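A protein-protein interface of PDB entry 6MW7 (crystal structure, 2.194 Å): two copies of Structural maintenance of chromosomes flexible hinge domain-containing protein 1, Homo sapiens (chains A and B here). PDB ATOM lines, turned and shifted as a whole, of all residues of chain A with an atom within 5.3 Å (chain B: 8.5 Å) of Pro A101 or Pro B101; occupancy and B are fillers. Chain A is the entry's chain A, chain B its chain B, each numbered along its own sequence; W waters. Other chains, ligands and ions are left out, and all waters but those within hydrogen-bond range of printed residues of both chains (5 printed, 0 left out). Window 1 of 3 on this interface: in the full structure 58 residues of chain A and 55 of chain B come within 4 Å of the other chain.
ND1 of His B102 is in hydrogen-bond range of N of Asp B104, 3.0 Å away. The backbone carbonyl oxygen of Pro A101 lies within hydrogen-bond range of the side-chain hydroxyl of Tyr A265. The side-chain hydroxyl (OH) of Tyr A265 lies close to the backbone NH (N) of Tyr A103. The backbone carbonyl oxygen (O) of His B102 sits at hydrogen-bond distance from the side-chain hydroxyl (OG1) of Thr B105, 2.7 Å away. OH of Tyr A265 sits at hydrogen-bond distance from O of His A102, 3.2 Å away. The backbone carbonyl oxygen (O) of Pro B101 is in hydrogen-bond range of the side-chain hydroxyl (OH) of Tyr B265.
Pro A101 touches three residues of chain B. Of the printed residues of chain A, Val B181 touches Phe A99 (3.97 Å), Leu A100 (3.2 Å) and His A102 (3.6 Å). Printed residues of chain A within 4 Å of Tyr B265: Phe A99 (2.9 Å), Leu A100 (3.5 Å) and Pro A101 (3.5 Å). Printed residues of chain B within 4 Å of His A102: Val B181 (3.6 Å) and Tyr B182 (3.0 Å). Of the printed residues of chain B, Tyr A265 touches Asp B98 (3.2 Å), Phe B99 (2.8 Å), Leu B100 (3.8 Å) and Pro B101 (3.6 Å). Phe B254 touches none of the printed residues of chain A. The nearest residue of chain A that does not touch Pro B101 is Val A181 (4.2 Å). The nearest printed residue of chain A that does not touch Tyr B265 is Tyr A182 (6.4 Å).
Water W5 bridges the guanidinium group of Arg B183 (2.7 Å) and the backbone carbonyl oxygen of Thr A105 (3.0 Å). Water W3 lies within hydrogen-bond range of O of Ala B180 (2.8 Å), N of Tyr B182 (2.8 Å) and O of Phe A99 (3.1 Å). Water W2 bridges the backbone NH (N) of Tyr A182 (2.9 Å) and the backbone carbonyl oxygen (O) of Phe B99 (3.0 Å). Water W1 lies within hydrogen-bond range of the side-chain hydroxyl of Tyr A182 and the side-chain hydroxyl of Tyr B182. Water W4 bridges OH of Tyr A182 (3.3 Å) and NH2 of Arg B183 (3.3 Å).
Among the printed residues, merely in contact across the chains: Phe A99 with Ala B180 (3.7 Å), Phe A99 with Val B181 (3.97 Å), Phe A99 with Ser B266 (3.9 Å), Leu A100 with Leu B100 (3.7 Å), Leu A100 with Val B181 (3.2 Å), Leu A100 with Tyr B265 (3.5 Å), Pro A101 with Pro B101 (3.97 Å), Pro A101 with Tyr B182 (3.9 Å), Pro A101 with Tyr B265 (3.5 Å), His A102 with Val B181 (3.6 Å), Thr A105 with Thr B105 (3.8 Å), Thr A105 with Tyr B182 (3.6 Å), Thr A105 with Arg B183 (3.7 Å), Val A181 with Leu B100 (3.3 Å), Val A181 with His B102 (3.6 Å), Tyr A182 with Pro B101 (3.9 Å), Tyr A182 with Thr B105 (3.6 Å), Tyr A265 with Asp B98 (3.2 Å), Tyr A265 with Leu B100 (3.8 Å) and Tyr A265 with Pro B101 (3.6 Å).
Phe A99 touches Val B181, but with the chains exchanged Val A181 does not touch Phe B99 (4.03 Å). Leu A100 touches Tyr B265, and with the chains exchanged Tyr A265 touches Leu B100. Pro A101 touches Tyr B265, and with the chains exchanged Tyr A265 touches Pro B101. His A102 touches Tyr B182, and with the chains exchanged Tyr A182 touches His B102. 9 positions are printed for both chains. Of the 24 pairs that touch across the chains among the printed residues, 19 have their exchanged pair printed and touching as well.
The backbone NH of Phe A99 sits at hydrogen-bond distance from the backbone carbonyl oxygen of Tyr B265. The backbone NH (N) of Phe B99 sits at hydrogen-bond distance from the backbone carbonyl oxygen (O) of Tyr A265 (2.8 Å). The backbone NH of His B102 sits at hydrogen-bond distance from the backbone carbonyl oxygen of Tyr A182. N of His A102 lies within hydrogen-bond range of O of Tyr B182 (3.0 Å).
Of the 19 printed residues of chain B, 12 touch a printed residue of chain A. Of the 9 printed residues of chain A, 8 touch a printed residue of chain B. Hydrophobic or aromatic side chains of chain A within 4 Å of the printed part of chain B: Phe A99, Leu A100, Pro A101, His A102, Val A181, Tyr A182 and Tyr A265. Among the printed residues, 24 pairs touch across the chains.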
ATOM      1  N   PHE A  99      -7.675  -4.786  26.864  1.00  0.00           N
ATOM      2  CA  PHE A  99      -8.590  -3.885  27.564  1.00  0.00           C
ATOM      3  C   PHE A  99      -8.085  -2.447  27.473  1.00  0.00           C
ATOM      4  O   PHE A  99      -7.927  -1.747  28.474  1.00  0.00           O
ATOM      5  CB  PHE A  99      -8.802  -4.331  29.014  1.00  0.00           C
ATOM      6  CG  PHE A  99      -7.534  -4.643  29.769  1.00  0.00           C
ATOM      7  CD1 PHE A  99      -6.964  -3.706  30.613  1.00  0.00           C
ATOM      8  CD2 PHE A  99      -6.937  -5.891  29.666  1.00  0.00           C
ATOM      9  CE1 PHE A  99      -5.810  -3.995  31.320  1.00  0.00           C
ATOM     10  CE2 PHE A  99      -5.779  -6.186  30.371  1.00  0.00           C
ATOM     11  CZ  PHE A  99      -5.217  -5.237  31.200  1.00  0.00           C
ATOM     12  N   LEU A 100      -7.842  -1.993  26.246  1.00  0.00           N
ATOM     13  CA  LEU A 100      -7.496  -0.599  26.018  1.00  0.00           C
ATOM     14  C   LEU A 100      -8.594   0.310  26.569  1.00  0.00           C
ATOM     15  O   LEU A 100      -9.782   0.044  26.352  1.00  0.00           O
ATOM     16  CB  LEU A 100      -7.323  -0.321  24.522  1.00  0.00           C
ATOM     17  CG  LEU A 100      -5.941  -0.339  23.865  1.00  0.00           C
ATOM     18  CD1 LEU A 100      -6.057   0.189  22.439  1.00  0.00           C
ATOM     19  CD2 LEU A 100      -4.926   0.476  24.640  1.00  0.00           C
ATOM     20  N   PRO A 101      -8.244   1.388  27.270  1.00  0.00           N
ATOM     21  CA  PRO A 101      -9.274   2.351  27.684  1.00  0.00           C
ATOM     22  C   PRO A 101     -10.076   2.858  26.493  1.00  0.00           C
ATOM     23  O   PRO A 101      -9.547   3.052  25.398  1.00  0.00           O
ATOM     24  CB  PRO A 101      -8.466   3.477  28.339  1.00  0.00           C
ATOM     25  CG  PRO A 101      -7.189   2.845  28.765  1.00  0.00           C
ATOM     26  CD  PRO A 101      -6.914   1.725  27.807  1.00  0.00           C
ATOM     27  N   HIS A 102     -11.372   3.053  26.717  1.00  0.00           N
ATOM     28  CA  HIS A 102     -12.241   3.635  25.705  1.00  0.00           C
ATOM     29  C   HIS A 102     -11.878   5.104  25.505  1.00  0.00           C
ATOM     30  O   HIS A 102     -11.509   5.800  26.456  1.00  0.00           O
ATOM     31  CB  HIS A 102     -13.701   3.494  26.137  1.00  0.00           C
ATOM     32  CG  HIS A 102     -14.695   3.850  25.077  1.00  0.00           C
ATOM     33  ND1 HIS A 102     -15.096   5.145  24.837  1.00  0.00           N
ATOM     34  CD2 HIS A 102     -15.390   3.076  24.210  1.00  0.00           C
ATOM     35  CE1 HIS A 102     -15.983   5.158  23.859  1.00  0.00           C
ATOM     36  NE2 HIS A 102     -16.181   3.914  23.462  1.00  0.00           N
ATOM     37  N   TYR A 103     -11.974   5.579  24.259  1.00  0.00           N
ATOM     38  CA  TYR A 103     -11.517   6.935  23.961  1.00  0.00           C
ATOM     39  C   TYR A 103     -12.291   7.993  24.736  1.00  0.00           C
ATOM     40  O   TYR A 103     -11.810   9.123  24.865  1.00  0.00           O
ATOM     41  CB  TYR A 103     -11.592   7.219  22.454  1.00  0.00           C
ATOM     42  CG  TYR A 103     -12.982   7.235  21.851  1.00  0.00           C
ATOM     43  CD1 TYR A 103     -13.839   8.308  22.052  1.00  0.00           C
ATOM     44  CD2 TYR A 103     -13.422   6.192  21.046  1.00  0.00           C
ATOM     45  CE1 TYR A 103     -15.104   8.330  21.490  1.00  0.00           C
ATOM     46  CE2 TYR A 103     -14.685   6.207  20.477  1.00  0.00           C
ATOM     47  CZ  TYR A 103     -15.521   7.278  20.703  1.00  0.00           C
ATOM     48  OH  TYR A 103     -16.778   7.301  20.144  1.00  0.00           O
ATOM     49  N   THR A 105     -12.271   8.050  27.669  1.00  0.00           N
ATOM     50  CA  THR A 105     -11.274   8.426  28.667  1.00  0.00           C
ATOM     51  C   THR A 105     -10.795   9.854  28.446  1.00  0.00           C
ATOM     52  O   THR A 105     -10.468  10.559  29.407  1.00  0.00           O
ATOM     53  CB  THR A 105     -10.096   7.448  28.616  1.00  0.00           C
ATOM     54  OG1 THR A 105     -10.540   6.143  29.008  1.00  0.00           O
ATOM     55  CG2 THR A 105      -8.959   7.889  29.535  1.00  0.00           C
ATOM     56  N   VAL A 181      -1.076  12.006  26.160  1.00  0.00           N
ATOM     57  CA  VAL A 181      -1.180  10.796  26.969  1.00  0.00           C
ATOM     58  C   VAL A 181      -1.914  11.143  28.261  1.00  0.00           C
ATOM     59  O   VAL A 181      -1.409  11.899  29.092  1.00  0.00           O
ATOM     60  CB  VAL A 181       0.198  10.190  27.264  1.00  0.00           C
ATOM     61  CG1 VAL A 181       0.062   8.961  28.159  1.00  0.00           C
ATOM     62  CG2 VAL A 181       0.902   9.822  25.970  1.00  0.00           C
ATOM     63  N   TYR A 182      -3.101  10.573  28.435  1.00  0.00           N
ATOM     64  CA  TYR A 182      -3.862  10.768  29.661  1.00  0.00           C
ATOM     65  C   TYR A 182      -3.114  10.182  30.856  1.00  0.00           C
ATOM     66  O   TYR A 182      -2.607   9.058  30.796  1.00  0.00           O
ATOM     67  CB  TYR A 182      -5.238  10.117  29.517  1.00  0.00           C
ATOM     68  CG  TYR A 182      -6.280  10.661  30.462  1.00  0.00           C
ATOM     69  CD1 TYR A 182      -6.844  11.913  30.255  1.00  0.00           C
ATOM     70  CD2 TYR A 182      -6.711   9.923  31.556  1.00  0.00           C
ATOM     71  CE1 TYR A 182      -7.801  12.418  31.118  1.00  0.00           C
ATOM     72  CE2 TYR A 182      -7.668  10.416  32.420  1.00  0.00           C
ATOM     73  CZ  TYR A 182      -8.212  11.665  32.199  1.00  0.00           C
ATOM     74  OH  TYR A 182      -9.166  12.155  33.061  1.00  0.00           O
ATOM     75  N   TYR A 265      -5.727   5.220  19.389  1.00  0.00           N
ATOM     76  CA  TYR A 265      -4.775   6.177  19.936  1.00  0.00           C
ATOM     77  C   TYR A 265      -3.547   6.351  19.045  1.00  0.00           C
ATOM     78  O   TYR A 265      -2.435   6.558  19.540  1.00  0.00           O
ATOM     79  CB  TYR A 265      -4.365   5.763  21.345  1.00  0.00           C
ATOM     80  CG  TYR A 265      -5.530   5.738  22.301  1.00  0.00           C
ATOM     81  CD1 TYR A 265      -6.087   6.917  22.769  1.00  0.00           C
ATOM     82  CD2 TYR A 265      -6.082   4.539  22.724  1.00  0.00           C
ATOM     83  CE1 TYR A 265      -7.156   6.908  23.637  1.00  0.00           C
ATOM     84  CE2 TYR A 265      -7.153   4.516  23.595  1.00  0.00           C
ATOM     85  CZ  TYR A 265      -7.687   5.703  24.049  1.00  0.00           C
ATOM     86  OH  TYR A 265      -8.752   5.681  24.912  1.00  0.00           O
ATOM     87  N   ASP B  98       1.730   7.544  18.664  1.00  0.00           N
ATOM     88  CA  ASP B  98       0.763   6.844  19.497  1.00  0.00           C
ATOM     89  C   ASP B  98       0.657   7.573  20.829  1.00  0.00           C
ATOM     90  O   ASP B  98       1.661   8.055  21.360  1.00  0.00           O
ATOM     91  CB  ASP B  98       1.177   5.390  19.732  1.00  0.00           C
ATOM     92  CG  ASP B  98       1.398   4.628  18.439  1.00  0.00           C
ATOM     93  OD1 ASP B  98       0.519   4.682  17.553  1.00  0.00           O
ATOM     94  OD2 ASP B  98       2.456   3.977  18.308  1.00  0.00           O
ATOM     95  N   PHE B  99      -0.559   7.660  21.365  1.00  0.00           N
ATOM     96  CA  PHE B  99      -0.796   8.316  22.645  1.00  0.00           C
ATOM     97  C   PHE B  99      -1.763   7.476  23.482  1.00  0.00           C
ATOM     98  O   PHE B  99      -2.806   7.936  23.936  1.00  0.00           O
ATOM     99  CB  PHE B  99      -1.317   9.739  22.441  1.00  0.00           C
ATOM    100  CG  PHE B  99      -2.437   9.843  21.439  1.00  0.00           C
ATOM    101  CD1 PHE B  99      -2.166   9.976  20.085  1.00  0.00           C
ATOM    102  CD2 PHE B  99      -3.757   9.822  21.849  1.00  0.00           C
ATOM    103  CE1 PHE B  99      -3.193  10.077  19.162  1.00  0.00           C
ATOM    104  CE2 PHE B  99      -4.789   9.922  20.931  1.00  0.00           C
ATOM    105  CZ  PHE B  99      -4.506  10.051  19.587  1.00  0.00           C
ATOM    106  N   LEU B 100      -1.406   6.214  23.697  1.00  0.00           N
ATOM    107  CA  LEU B 100      -2.201   5.359  24.566  1.00  0.00           C
ATOM    108  C   LEU B 100      -2.229   5.944  25.978  1.00  0.00           C
ATOM    109  O   LEU B 100      -1.189   6.382  26.485  1.00  0.00           O
ATOM    110  CB  LEU B 100      -1.623   3.945  24.621  1.00  0.00           C
ATOM    111  CG  LEU B 100      -1.966   2.974  23.490  1.00  0.00           C
ATOM    112  CD1 LEU B 100      -1.393   3.437  22.162  1.00  0.00           C
ATOM    113  CD2 LEU B 100      -1.454   1.589  23.841  1.00  0.00           C
ATOM    114  N   PRO B 101      -3.381   5.955  26.646  1.00  0.00           N
ATOM    115  CA  PRO B 101      -3.407   6.399  28.044  1.00  0.00           C
ATOM    116  C   PRO B 101      -2.396   5.638  28.888  1.00  0.00           C
ATOM    117  O   PRO B 101      -2.176   4.441  28.699  1.00  0.00           O
ATOM    118  CB  PRO B 101      -4.843   6.100  28.483  1.00  0.00           C
ATOM    119  CG  PRO B 101      -5.635   6.154  27.225  1.00  0.00           C
ATOM    120  CD  PRO B 101      -4.728   5.605  26.159  1.00  0.00           C
ATOM    121  N   HIS B 102      -1.763   6.350  29.815  1.00  0.00           N
ATOM    122  CA  HIS B 102      -0.868   5.713  30.767  1.00  0.00           C
ATOM    123  C   HIS B 102      -1.682   4.858  31.734  1.00  0.00           C
ATOM    124  O   HIS B 102      -2.846   5.150  32.020  1.00  0.00           O
ATOM    125  CB  HIS B 102      -0.060   6.772  31.520  1.00  0.00           C
ATOM    126  CG  HIS B 102       1.005   6.211  32.408  1.00  0.00           C
ATOM    127  ND1 HIS B 102       0.751   5.768  33.686  1.00  0.00           N
ATOM    128  CD2 HIS B 102       2.330   6.033  32.205  1.00  0.00           C
ATOM    129  CE1 HIS B 102       1.873   5.331  34.231  1.00  0.00           C
ATOM    130  NE2 HIS B 102       2.846   5.483  33.354  1.00  0.00           N
ATOM    131  N   TYR B 103      -1.072   3.775  32.226  1.00  0.00           N
ATOM    132  CA  TYR B 103      -1.834   2.811  33.015  1.00  0.00           C
ATOM    133  C   TYR B 103      -2.312   3.388  34.343  1.00  0.00           C
ATOM    134  O   TYR B 103      -3.229   2.828  34.950  1.00  0.00           O
ATOM    135  CB  TYR B 103      -1.021   1.529  33.250  1.00  0.00           C
ATOM    136  CG  TYR B 103       0.256   1.672  34.057  1.00  0.00           C
ATOM    137  CD1 TYR B 103       0.222   1.869  35.432  1.00  0.00           C
ATOM    138  CD2 TYR B 103       1.498   1.564  33.447  1.00  0.00           C
ATOM    139  CE1 TYR B 103       1.389   1.985  36.169  1.00  0.00           C
ATOM    140  CE2 TYR B 103       2.668   1.676  34.176  1.00  0.00           C
ATOM    141  CZ  TYR B 103       2.608   1.885  35.537  1.00  0.00           C
ATOM    142  OH  TYR B 103       3.771   1.997  36.266  1.00  0.00           O
ATOM    143  N   ASP B 104      -1.731   4.499  34.801  1.00  0.00           N
ATOM    144  CA  ASP B 104      -2.289   5.210  35.946  1.00  0.00           C
ATOM    145  C   ASP B 104      -3.709   5.687  35.673  1.00  0.00           C
ATOM    146  O   ASP B 104      -4.417   6.066  36.612  1.00  0.00           O
ATOM    147  CB  ASP B 104      -1.405   6.399  36.325  1.00  0.00           C
ATOM    148  CG  ASP B 104      -0.153   5.986  37.077  1.00  0.00           C
ATOM    149  OD1 ASP B 104      -0.117   4.861  37.619  1.00  0.00           O
ATOM    150  OD2 ASP B 104       0.797   6.795  37.137  1.00  0.00           O
ATOM    151  N   THR B 105      -4.138   5.687  34.407  1.00  0.00           N
ATOM    152  CA  THR B 105      -5.554   5.856  34.103  1.00  0.00           C
ATOM    153  C   THR B 105      -6.399   4.875  34.901  1.00  0.00           C
ATOM    154  O   THR B 105      -7.555   5.168  35.224  1.00  0.00           O
ATOM    155  CB  THR B 105      -5.784   5.683  32.598  1.00  0.00           C
ATOM    156  OG1 THR B 105      -5.031   6.673  31.882  1.00  0.00           O
ATOM    157  CG2 THR B 105      -7.260   5.831  32.241  1.00  0.00           C
ATOM    158  N   LEU B 106      -5.838   3.713  35.234  1.00  0.00           N
ATOM    159  CA  LEU B 106      -6.478   2.745  36.114  1.00  0.00           C
ATOM    160  C   LEU B 106      -5.930   2.804  37.536  1.00  0.00           C
ATOM    161  O   LEU B 106      -6.700   2.918  38.493  1.00  0.00           O
ATOM    162  CB  LEU B 106      -6.297   1.328  35.552  1.00  0.00           C
ATOM    163  CG  LEU B 106      -7.116   0.961  34.314  1.00  0.00           C
ATOM    164  CD1 LEU B 106      -6.516  -0.250  33.613  1.00  0.00           C
ATOM    165  CD2 LEU B 106      -8.563   0.691  34.689  1.00  0.00           C
ATOM    166  N   ASN B 178     -14.982  -6.445  29.250  1.00  0.00           N
ATOM    167  CA  ASN B 178     -15.558  -5.106  29.194  1.00  0.00           C
ATOM    168  C   ASN B 178     -15.349  -4.359  30.502  1.00  0.00           C
ATOM    169  O   ASN B 178     -15.055  -3.158  30.499  1.00  0.00           O
ATOM    170  CB  ASN B 178     -17.046  -5.192  28.860  1.00  0.00           C
ATOM    171  CG  ASN B 178     -17.295  -5.529  27.408  1.00  0.00           C
ATOM    172  OD1 ASN B 178     -16.358  -5.681  26.621  1.00  0.00           O
ATOM    173  ND2 ASN B 178     -18.562  -5.656  27.042  1.00  0.00           N
ATOM    174  N   ALA B 180     -12.914  -4.412  32.408  1.00  0.00           N
ATOM    175  CA  ALA B 180     -11.549  -3.911  32.490  1.00  0.00           C
ATOM    176  C   ALA B 180     -11.289  -2.719  31.576  1.00  0.00           C
ATOM    177  O   ALA B 180     -10.194  -2.148  31.632  1.00  0.00           O
ATOM    178  CB  ALA B 180     -10.562  -5.029  32.156  1.00  0.00           C
ATOM    179  N   VAL B 181     -12.251  -2.328  30.747  1.00  0.00           N
ATOM    180  CA  VAL B 181     -12.090  -1.189  29.849  1.00  0.00           C
ATOM    181  C   VAL B 181     -12.563   0.062  30.582  1.00  0.00           C
ATOM    182  O   VAL B 181     -13.752   0.213  30.875  1.00  0.00           O
ATOM    183  CB  VAL B 181     -12.859  -1.390  28.539  1.00  0.00           C
ATOM    184  CG1 VAL B 181     -12.744  -0.151  27.657  1.00  0.00           C
ATOM    185  CG2 VAL B 181     -12.336  -2.604  27.801  1.00  0.00           C
ATOM    186  N   TYR B 182     -11.632   0.965  30.870  1.00  0.00           N
ATOM    187  CA  TYR B 182     -11.985   2.226  31.507  1.00  0.00           C
ATOM    188  C   TYR B 182     -12.914   3.036  30.612  1.00  0.00           C
ATOM    189  O   TYR B 182     -12.671   3.178  29.409  1.00  0.00           O
ATOM    190  CB  TYR B 182     -10.719   3.024  31.820  1.00  0.00           C
ATOM    191  CG  TYR B 182     -10.926   4.082  32.879  1.00  0.00           C
ATOM    192  CD1 TYR B 182     -11.116   3.728  34.209  1.00  0.00           C
ATOM    193  CD2 TYR B 182     -10.931   5.433  32.555  1.00  0.00           C
ATOM    194  CE1 TYR B 182     -11.308   4.684  35.183  1.00  0.00           C
ATOM    195  CE2 TYR B 182     -11.122   6.401  33.529  1.00  0.00           C
ATOM    196  CZ  TYR B 182     -11.311   6.019  34.840  1.00  0.00           C
ATOM    197  OH  TYR B 182     -11.501   6.974  35.810  1.00  0.00           O
ATOM    198  N   ARG B 183     -13.984   3.564  31.205  1.00  0.00           N
ATOM    199  CA  ARG B 183     -14.984   4.400  30.542  1.00  0.00           C
ATOM    200  C   ARG B 183     -15.861   3.628  29.566  1.00  0.00           C
ATOM    201  O   ARG B 183     -16.615   4.249  28.806  1.00  0.00           O
ATOM    202  CB  ARG B 183     -14.348   5.588  29.812  1.00  0.00           C
ATOM    203  CG  ARG B 183     -13.858   6.683  30.734  1.00  0.00           C
ATOM    204  CD  ARG B 183     -14.955   7.681  31.079  1.00  0.00           C
ATOM    205  NE  ARG B 183     -14.465   8.711  31.990  1.00  0.00           N
ATOM    206  CZ  ARG B 183     -15.234   9.586  32.632  1.00  0.00           C
ATOM    207  NH1 ARG B 183     -16.551   9.567  32.477  1.00  0.00           N
ATOM    208  NH2 ARG B 183     -14.682  10.481  33.436  1.00  0.00           N
ATOM    209  N   LEU B 184     -15.799   2.299  29.562  1.00  0.00           N
ATOM    210  CA  LEU B 184     -16.748   1.499  28.794  1.00  0.00           C
ATOM    211  C   LEU B 184     -18.014   1.338  29.626  1.00  0.00           C
ATOM    212  O   LEU B 184     -18.007   0.655  30.656  1.00  0.00           O
ATOM    213  CB  LEU B 184     -16.145   0.146  28.425  1.00  0.00           C
ATOM    214  CG  LEU B 184     -17.025  -0.776  27.578  1.00  0.00           C
ATOM    215  CD1 LEU B 184     -17.423  -0.111  26.267  1.00  0.00           C
ATOM    216  CD2 LEU B 184     -16.306  -2.082  27.306  1.00  0.00           C
ATOM    217  N   PHE B 254       1.111  -4.035  35.846  1.00  0.00           N
ATOM    218  CA  PHE B 254       1.411  -2.948  34.920  1.00  0.00           C
ATOM    219  C   PHE B 254       2.891  -2.590  34.962  1.00  0.00           C
ATOM    220  O   PHE B 254       3.508  -2.346  33.919  1.00  0.00           O
ATOM    221  CB  PHE B 254       0.563  -1.718  35.245  1.00  0.00           C
ATOM    222  CG  PHE B 254      -0.879  -1.843  34.843  1.00  0.00           C
ATOM    223  CD1 PHE B 254      -1.226  -2.115  33.533  1.00  0.00           C
ATOM    224  CD2 PHE B 254      -1.889  -1.662  35.772  1.00  0.00           C
ATOM    225  CE1 PHE B 254      -2.551  -2.224  33.159  1.00  0.00           C
ATOM    226  CE2 PHE B 254      -3.218  -1.767  35.405  1.00  0.00           C
ATOM    227  CZ  PHE B 254      -3.549  -2.045  34.095  1.00  0.00           C
ATOM    228  N   ILE B 264       0.682  -2.852  27.460  1.00  0.00           N
ATOM    229  CA  ILE B 264       0.226  -2.443  28.785  1.00  0.00           C
ATOM    230  C   ILE B 264      -1.178  -2.963  29.065  1.00  0.00           C
ATOM    231  O   ILE B 264      -1.474  -3.409  30.179  1.00  0.00           O
ATOM    232  CB  ILE B 264       0.303  -0.909  28.916  1.00  0.00           C
ATOM    233  CG1 ILE B 264       1.765  -0.447  28.920  1.00  0.00           C
ATOM    234  CG2 ILE B 264      -0.421  -0.416  30.168  1.00  0.00           C
ATOM    235  CD1 ILE B 264       2.590  -0.941  30.101  1.00  0.00           C
ATOM    236  N   TYR B 265      -2.064  -2.911  28.075  1.00  0.00           N
ATOM    237  CA  TYR B 265      -3.457  -3.309  28.261  1.00  0.00           C
ATOM    238  C   TYR B 265      -3.751  -4.678  27.662  1.00  0.00           C
ATOM    239  O   TYR B 265      -4.839  -4.921  27.133  1.00  0.00           O
ATOM    240  CB  TYR B 265      -4.380  -2.245  27.679  1.00  0.00           C
ATOM    241  CG  TYR B 265      -4.211  -0.907  28.361  1.00  0.00           C
ATOM    242  CD1 TYR B 265      -4.763  -0.674  29.614  1.00  0.00           C
ATOM    243  CD2 TYR B 265      -3.488   0.117  27.764  1.00  0.00           C
ATOM    244  CE1 TYR B 265      -4.610   0.540  30.246  1.00  0.00           C
ATOM    245  CE2 TYR B 265      -3.331   1.336  28.385  1.00  0.00           C
ATOM    246  CZ  TYR B 265      -3.892   1.546  29.626  1.00  0.00           C
ATOM    247  OH  TYR B 265      -3.728   2.764  30.242  1.00  0.00           O
ATOM    248  N   SER B 266      -2.788  -5.591  27.742  1.00  0.00           N
ATOM    249  CA  SER B 266      -2.987  -6.989  27.389  1.00  0.00           C
ATOM    250  C   SER B 266      -2.756  -7.857  28.618  1.00  0.00           C
ATOM    251  O   SER B 266      -1.813  -7.632  29.381  1.00  0.00           O
ATOM    252  CB  SER B 266      -2.048  -7.417  26.258  1.00  0.00           C
ATOM    253  OG  SER B 266      -2.439  -6.837  25.026  1.00  0.00           O
HETATM  254  O   HOH W   1     -10.466   9.888  34.874  1.00  0.00           O
HETATM  255  O   HOH W   2      -4.315   9.366  26.097  1.00  0.00           O
HETATM  256  O   HOH W   3      -8.992   0.135  30.641  1.00  0.00           O
HETATM  257  O   HOH W   4     -12.144  12.383  34.380  1.00  0.00           O
HETATM  258  O   HOH W   5     -11.948   9.764  31.936  1.00  0.00           O
